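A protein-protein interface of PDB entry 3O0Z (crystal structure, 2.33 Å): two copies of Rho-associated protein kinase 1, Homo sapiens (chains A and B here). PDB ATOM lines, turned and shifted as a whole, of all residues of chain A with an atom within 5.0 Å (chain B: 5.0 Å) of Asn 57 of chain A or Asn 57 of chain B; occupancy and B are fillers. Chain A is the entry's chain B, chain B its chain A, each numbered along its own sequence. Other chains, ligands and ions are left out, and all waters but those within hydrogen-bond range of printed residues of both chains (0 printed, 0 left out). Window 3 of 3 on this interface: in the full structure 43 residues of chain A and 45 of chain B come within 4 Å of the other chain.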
ATOM      1  N   LEU A  53      16.471 -17.857  19.269  1.00  0.00           N
ATOM      2  CA  LEU A  53      16.092 -16.481  19.026  1.00  0.00           C
ATOM      3  C   LEU A  53      16.844 -15.965  17.804  1.00  0.00           C
ATOM      4  O   LEU A  53      16.271 -15.279  16.968  1.00  0.00           O
ATOM      5  CB  LEU A  53      16.389 -15.594  20.232  1.00  0.00           C
ATOM      6  CG  LEU A  53      16.250 -14.095  19.926  1.00  0.00           C
ATOM      7  CD1 LEU A  53      14.817 -13.599  20.139  1.00  0.00           C
ATOM      8  CD2 LEU A  53      17.242 -13.236  20.716  1.00  0.00           C
ATOM      9  N   GLN A  54      18.128 -16.290  17.689  1.00  0.00           N
ATOM     10  CA  GLN A  54      18.901 -15.790  16.551  1.00  0.00           C
ATOM     11  C   GLN A  54      18.420 -16.369  15.232  1.00  0.00           C
ATOM     12  O   GLN A  54      18.526 -15.715  14.203  1.00  0.00           O
ATOM     13  CB  GLN A  54      20.397 -16.049  16.717  1.00  0.00           C
ATOM     14  CG  GLN A  54      21.110 -15.020  17.590  1.00  0.00           C
ATOM     15  CD  GLN A  54      22.476 -15.505  18.061  1.00  0.00           C
ATOM     16  OE1 GLN A  54      23.317 -15.897  17.253  1.00  0.00           O
ATOM     17  NE2 GLN A  54      22.696 -15.483  19.372  1.00  0.00           N
ATOM     18  N   GLU A  55      17.913 -17.599  15.275  1.00  0.00           N
ATOM     19  CA  GLU A  55      17.390 -18.270  14.100  1.00  0.00           C
ATOM     20  C   GLU A  55      16.112 -17.598  13.598  1.00  0.00           C
ATOM     21  O   GLU A  55      16.011 -17.262  12.424  1.00  0.00           O
ATOM     22  CB  GLU A  55      17.105 -19.734  14.402  1.00  0.00           C
ATOM     23  CG  GLU A  55      18.025 -20.695  13.684  1.00  0.00           C
ATOM     24  CD  GLU A  55      17.827 -20.727  12.174  1.00  0.00           C
ATOM     25  OE1 GLU A  55      16.919 -21.456  11.684  1.00  0.00           O
ATOM     26  OE2 GLU A  55      18.614 -20.045  11.480  1.00  0.00           O
ATOM     27  N   ARG A  56      15.141 -17.416  14.490  1.00  0.00           N
ATOM     28  CA  ARG A  56      13.937 -16.678  14.155  1.00  0.00           C
ATOM     29  C   ARG A  56      14.276 -15.346  13.500  1.00  0.00           C
ATOM     30  O   ARG A  56      13.780 -15.060  12.419  1.00  0.00           O
ATOM     31  CB  ARG A  56      13.051 -16.473  15.374  1.00  0.00           C
ATOM     32  CG  ARG A  56      12.464 -17.755  15.904  1.00  0.00           C
ATOM     33  CD  ARG A  56      11.558 -17.464  17.083  1.00  0.00           C
ATOM     34  NE  ARG A  56      11.632 -18.509  18.103  1.00  0.00           N
ATOM     35  CZ  ARG A  56      11.072 -18.420  19.307  1.00  0.00           C
ATOM     36  NH1 ARG A  56      10.395 -17.327  19.649  1.00  0.00           N
ATOM     37  NH2 ARG A  56      11.191 -19.424  20.168  1.00  0.00           N
ATOM     38  N   ASN A  57      15.129 -14.536  14.124  1.00  0.00           N
ATOM     39  CA  ASN A  57      15.535 -13.296  13.466  1.00  0.00           C
ATOM     40  C   ASN A  57      15.970 -13.518  12.016  1.00  0.00           C
ATOM     41  O   ASN A  57      15.574 -12.773  11.127  1.00  0.00           O
ATOM     42  CB  ASN A  57      16.637 -12.565  14.234  1.00  0.00           C
ATOM     43  CG  ASN A  57      16.152 -12.005  15.556  1.00  0.00           C
ATOM     44  OD1 ASN A  57      16.955 -11.659  16.440  1.00  0.00           O
ATOM     45  ND2 ASN A  57      14.830 -11.933  15.716  1.00  0.00           N
ATOM     46  N   ARG A  58      16.779 -14.544  11.781  1.00  0.00           N
ATOM     47  CA  ARG A  58      17.335 -14.787  10.455  1.00  0.00           C
ATOM     48  C   ARG A  58      16.233 -15.095   9.458  1.00  0.00           C
ATOM     49  O   ARG A  58      16.234 -14.597   8.324  1.00  0.00           O
ATOM     50  CB  ARG A  58      18.310 -15.956  10.509  1.00  0.00           C
ATOM     51  CG  ARG A  58      18.916 -16.333   9.176  1.00  0.00           C
ATOM     52  CD  ARG A  58      19.611 -17.678   9.279  1.00  0.00           C
ATOM     53  NE  ARG A  58      19.332 -18.493   8.102  1.00  0.00           N
ATOM     54  CZ  ARG A  58      18.338 -19.376   8.007  1.00  0.00           C
ATOM     55  NH1 ARG A  58      17.508 -19.587   9.021  1.00  0.00           N
ATOM     56  NH2 ARG A  58      18.178 -20.060   6.888  1.00  0.00           N
ATOM     57  N   ILE A  59      15.303 -15.942   9.888  1.00  0.00           N
ATOM     58  CA  ILE A  59      14.183 -16.326   9.063  1.00  0.00           C
ATOM     59  C   ILE A  59      13.287 -15.114   8.792  1.00  0.00           C
ATOM     60  O   ILE A  59      12.929 -14.842   7.646  1.00  0.00           O
ATOM     61  CB  ILE A  59      13.351 -17.380   9.748  1.00  0.00           C
ATOM     62  CG1 ILE A  59      14.088 -18.700   9.740  1.00  0.00           C
ATOM     63  CG2 ILE A  59      11.988 -17.511   9.036  1.00  0.00           C
ATOM     64  CD1 ILE A  59      13.550 -19.660  10.762  1.00  0.00           C
ATOM     65  N   LEU A  60      12.920 -14.414   9.863  1.00  0.00           N
ATOM     66  CA  LEU A  60      12.221 -13.146   9.773  1.00  0.00           C
ATOM     67  C   LEU A  60      12.878 -12.228   8.765  1.00  0.00           C
ATOM     68  O   LEU A  60      12.228 -11.771   7.842  1.00  0.00           O
ATOM     69  CB  LEU A  60      12.170 -12.465  11.136  1.00  0.00           C
ATOM     70  CG  LEU A  60      10.761 -12.310  11.698  1.00  0.00           C
ATOM     71  CD1 LEU A  60       9.809 -13.347  11.132  1.00  0.00           C
ATOM     72  CD2 LEU A  60      10.797 -12.379  13.200  1.00  0.00           C
ATOM     73  N   GLU A  61      14.167 -11.947   8.929  1.00  0.00           N
ATOM     74  CA  GLU A  61      14.831 -11.016   8.006  1.00  0.00           C
ATOM     75  C   GLU A  61      14.822 -11.498   6.552  1.00  0.00           C
ATOM     76  O   GLU A  61      14.748 -10.691   5.619  1.00  0.00           O
ATOM     77  CB  GLU A  61      16.257 -10.695   8.468  1.00  0.00           C
ATOM     78  CG  GLU A  61      16.309  -9.764   9.683  1.00  0.00           C
ATOM     79  CD  GLU A  61      17.597  -9.899  10.526  1.00  0.00           C
ATOM     80  OE1 GLU A  61      17.908  -8.951  11.288  1.00  0.00           O
ATOM     81  OE2 GLU A  61      18.294 -10.942  10.440  1.00  0.00           O
ATOM     82  N   ASN A  62      14.889 -12.815   6.374  1.00  0.00           N
ATOM     83  CA  ASN A  62      14.946 -13.426   5.051  1.00  0.00           C
ATOM     84  C   ASN A  62      13.581 -13.456   4.396  1.00  0.00           C
ATOM     85  O   ASN A  62      13.447 -13.158   3.210  1.00  0.00           O
ATOM     86  CB  ASN A  62      15.452 -14.865   5.126  1.00  0.00           C
ATOM     87  CG  ASN A  62      16.965 -14.969   5.030  1.00  0.00           C
ATOM     88  OD1 ASN A  62      17.694 -13.972   5.106  1.00  0.00           O
ATOM     89  ND2 ASN A  62      17.441 -16.190   4.856  1.00  0.00           N
ATOM     90  N   GLU B  52      17.118  -6.196  25.422  1.00  0.00           N
ATOM     91  CA  GLU B  52      17.239  -5.468  24.158  1.00  0.00           C
ATOM     92  C   GLU B  52      16.942  -6.353  22.950  1.00  0.00           C
ATOM     93  O   GLU B  52      16.201  -5.946  22.044  1.00  0.00           O
ATOM     94  CB  GLU B  52      18.622  -4.853  23.994  1.00  0.00           C
ATOM     95  CG  GLU B  52      18.927  -3.713  24.941  1.00  0.00           C
ATOM     96  CD  GLU B  52      20.423  -3.433  25.054  1.00  0.00           C
ATOM     97  OE1 GLU B  52      21.223  -4.134  24.383  1.00  0.00           O
ATOM     98  OE2 GLU B  52      20.795  -2.514  25.821  1.00  0.00           O
ATOM     99  N   LEU B  53      17.522  -7.550  22.922  1.00  0.00           N
ATOM    100  CA  LEU B  53      17.299  -8.452  21.791  1.00  0.00           C
ATOM    101  C   LEU B  53      15.828  -8.852  21.649  1.00  0.00           C
ATOM    102  O   LEU B  53      15.335  -9.071  20.535  1.00  0.00           O
ATOM    103  CB  LEU B  53      18.204  -9.682  21.865  1.00  0.00           C
ATOM    104  CG  LEU B  53      19.701  -9.355  21.791  1.00  0.00           C
ATOM    105  CD1 LEU B  53      20.535 -10.628  21.657  1.00  0.00           C
ATOM    106  CD2 LEU B  53      20.000  -8.377  20.643  1.00  0.00           C
ATOM    107  N   GLN B  54      15.136  -8.928  22.779  1.00  0.00           N
ATOM    108  CA  GLN B  54      13.714  -9.244  22.796  1.00  0.00           C
ATOM    109  C   GLN B  54      12.884  -8.147  22.116  1.00  0.00           C
ATOM    110  O   GLN B  54      11.871  -8.419  21.478  1.00  0.00           O
ATOM    111  CB  GLN B  54      13.247  -9.416  24.238  1.00  0.00           C
ATOM    112  CG  GLN B  54      12.253 -10.525  24.408  1.00  0.00           C
ATOM    113  CD  GLN B  54      12.838 -11.850  24.001  1.00  0.00           C
ATOM    114  OE1 GLN B  54      12.672 -12.290  22.853  1.00  0.00           O
ATOM    115  NE2 GLN B  54      13.544 -12.502  24.941  1.00  0.00           N
ATOM    116  N   GLU B  55      13.341  -6.912  22.266  1.00  0.00           N
ATOM    117  CA  GLU B  55      12.669  -5.734  21.753  1.00  0.00           C
ATOM    118  C   GLU B  55      12.977  -5.495  20.263  1.00  0.00           C
ATOM    119  O   GLU B  55      12.096  -5.103  19.497  1.00  0.00           O
ATOM    120  CB  GLU B  55      13.074  -4.517  22.595  1.00  0.00           C
ATOM    121  CG  GLU B  55      12.432  -3.196  22.193  1.00  0.00           C
ATOM    122  CD  GLU B  55      10.936  -3.167  22.485  1.00  0.00           C
ATOM    123  OE1 GLU B  55      10.270  -2.193  22.063  1.00  0.00           O
ATOM    124  OE2 GLU B  55      10.428  -4.121  23.131  1.00  0.00           O
ATOM    125  N   ARG B  56      14.220  -5.726  19.852  1.00  0.00           N
ATOM    126  CA  ARG B  56      14.562  -5.666  18.437  1.00  0.00           C
ATOM    127  C   ARG B  56      13.784  -6.743  17.692  1.00  0.00           C
ATOM    128  O   ARG B  56      13.400  -6.557  16.545  1.00  0.00           O
ATOM    129  CB  ARG B  56      16.067  -5.858  18.216  1.00  0.00           C
ATOM    130  CG  ARG B  56      16.885  -4.583  18.339  1.00  0.00           C
ATOM    131  CD  ARG B  56      18.350  -4.895  18.692  1.00  0.00           C
ATOM    132  NE  ARG B  56      18.997  -3.760  19.352  1.00  0.00           N
ATOM    133  CZ  ARG B  56      19.921  -3.858  20.315  1.00  0.00           C
ATOM    134  NH1 ARG B  56      20.343  -5.055  20.751  1.00  0.00           N
ATOM    135  NH2 ARG B  56      20.430  -2.747  20.844  1.00  0.00           N
ATOM    136  N   ASN B  57      13.552  -7.873  18.348  1.00  0.00           N
ATOM    137  CA  ASN B  57      12.785  -8.945  17.734  1.00  0.00           C
ATOM    138  C   ASN B  57      11.304  -8.613  17.614  1.00  0.00           C
ATOM    139  O   ASN B  57      10.687  -8.878  16.594  1.00  0.00           O
ATOM    140  CB  ASN B  57      12.931 -10.223  18.529  1.00  0.00           C
ATOM    141  CG  ASN B  57      12.108 -11.346  17.967  1.00  0.00           C
ATOM    142  OD1 ASN B  57      12.617 -12.187  17.223  1.00  0.00           O
ATOM    143  ND2 ASN B  57      10.828 -11.378  18.321  1.00  0.00           N
ATOM    144  N   ARG B  58      10.729  -8.058  18.671  1.00  0.00           N
ATOM    145  CA  ARG B  58       9.341  -7.632  18.638  1.00  0.00           C
ATOM    146  C   ARG B  58       9.157  -6.693  17.447  1.00  0.00           C
ATOM    147  O   ARG B  58       8.207  -6.824  16.688  1.00  0.00           O
ATOM    148  CB  ARG B  58       8.982  -6.935  19.953  1.00  0.00           C
ATOM    149  CG  ARG B  58       7.589  -6.315  20.019  1.00  0.00           C
ATOM    150  CD  ARG B  58       7.446  -5.485  21.302  1.00  0.00           C
ATOM    151  NE  ARG B  58       6.637  -4.293  21.066  1.00  0.00           N
ATOM    152  CZ  ARG B  58       7.132  -3.108  20.721  1.00  0.00           C
ATOM    153  NH1 ARG B  58       8.439  -2.950  20.578  1.00  0.00           N
ATOM    154  NH2 ARG B  58       6.320  -2.080  20.516  1.00  0.00           N
ATOM    155  N   ILE B  59      10.101  -5.769  17.280  1.00  0.00           N
ATOM    156  CA  ILE B  59      10.089  -4.802  16.185  1.00  0.00           C
ATOM    157  C   ILE B  59      10.228  -5.460  14.817  1.00  0.00           C
ATOM    158  O   ILE B  59       9.483  -5.141  13.892  1.00  0.00           O
ATOM    159  CB  ILE B  59      11.187  -3.737  16.380  1.00  0.00           C
ATOM    160  CG1 ILE B  59      10.800  -2.806  17.529  1.00  0.00           C
ATOM    161  CG2 ILE B  59      11.399  -2.914  15.109  1.00  0.00           C
ATOM    162  CD1 ILE B  59      11.971  -2.054  18.131  1.00  0.00           C
ATOM    163  N   LEU B  60      11.173  -6.383  14.695  1.00  0.00           N
ATOM    164  CA  LEU B  60      11.356  -7.140  13.460  1.00  0.00           C
ATOM    165  C   LEU B  60      10.046  -7.796  13.017  1.00  0.00           C
ATOM    166  O   LEU B  60       9.683  -7.758  11.841  1.00  0.00           O
ATOM    167  CB  LEU B  60      12.392  -8.233  13.674  1.00  0.00           C
ATOM    168  CG  LEU B  60      13.532  -8.387  12.683  1.00  0.00           C
ATOM    169  CD1 LEU B  60      13.944  -9.840  12.654  1.00  0.00           C
ATOM    170  CD2 LEU B  60      13.121  -7.951  11.316  1.00  0.00           C
ATOM    171  N   GLU B  61       9.357  -8.405  13.977  1.00  0.00           N
ATOM    172  CA  GLU B  61       8.139  -9.156  13.726  1.00  0.00           C
ATOM    173  C   GLU B  61       7.055  -8.266  13.144  1.00  0.00           C
ATOM    174  O   GLU B  61       6.449  -8.596  12.128  1.00  0.00           O
ATOM    175  CB  GLU B  61       7.650  -9.788  15.029  1.00  0.00           C
ATOM    176  CG  GLU B  61       7.333 -11.268  14.913  1.00  0.00           C
ATOM    177  CD  GLU B  61       8.005 -12.088  15.997  1.00  0.00           C
ATOM    178  OE1 GLU B  61       8.374 -11.506  17.043  1.00  0.00           O
ATOM    179  OE2 GLU B  61       8.167 -13.313  15.803  1.00  0.00           O
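Among the printed residues, pairs that only touch across the chains: Leu 60 of chain A with Leu 60 of chain B (3.5 Å), Asn 57 of chain A with Leu 60 of chain B (3.7 Å), Leu 53 of chain A with Gln 54 of chain B (3.7 Å), Glu 61 of chain A with Leu 60 of chain B (3.8 Å), Leu 60 of chain A with Glu 61 of chain B (3.8 Å), Leu 53 of chain A with Leu 53 of chain B (3.9 Å) and Leu 53 of chain A with Asn 57 of chain B (3.9 Å).
Leu 53 of chain A touches Gln 54 of chain B, but with the chains exchanged Gln 54 of chain A does not touch Leu 53 of chain B (5.8 Å).
Leu 53 of chain A touches Asn 57 of chain B, but with the chains exchanged Asn 57 of chain A does not touch Leu 53 of chain B (5.1 Å).
Leu 60 of chain B touches its own counterpart, Leu 60 of chain A.
Leu 60 of chain A touches Glu 61 of chain B, and with the chains exchanged Glu 61 of chain A touches Leu 60 of chain B.
9 positions are printed for both chains.
Along chain B the printed residues that touch a printed residue of chain A span positions 53 to 61.
ND2 of Asn 57 of chain B is in hydrogen-bond range of OE1 of Glu 61 of chain B.
The side-chain amide nitrogen (ND2) of Asn 57 of chain A sits at hydrogen-bond distance from the side-chain amide oxygen (OD1) of Asn 57 of chain B (2.7 Å).
Of chain B, only Asn 57 (2.7 Å) and Leu 60 (3.7 Å) come within 4 Å of Asn 57 of chain A.
Of chain A, only Leu 53 (3.9 Å) and Asn 57 (2.7 Å) come within 4 Å of Asn 57 of chain B.
Of the printed residues of chain A, Gln 54 of chain B touches Leu 53 (3.7 Å).
Of the printed residues of chain B, Leu 53 of chain A touches Leu 53 (3.9 Å), Gln 54 (3.7 Å) and Asn 57 (3.9 Å).
The nearest residue of chain A that does not touch Asn 57 of chain B is Leu 60 of chain A (4.4 Å).
The nearest printed residue of chain A that does not touch Gln 54 of chain B is Arg 56 of chain A (6.4 Å).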
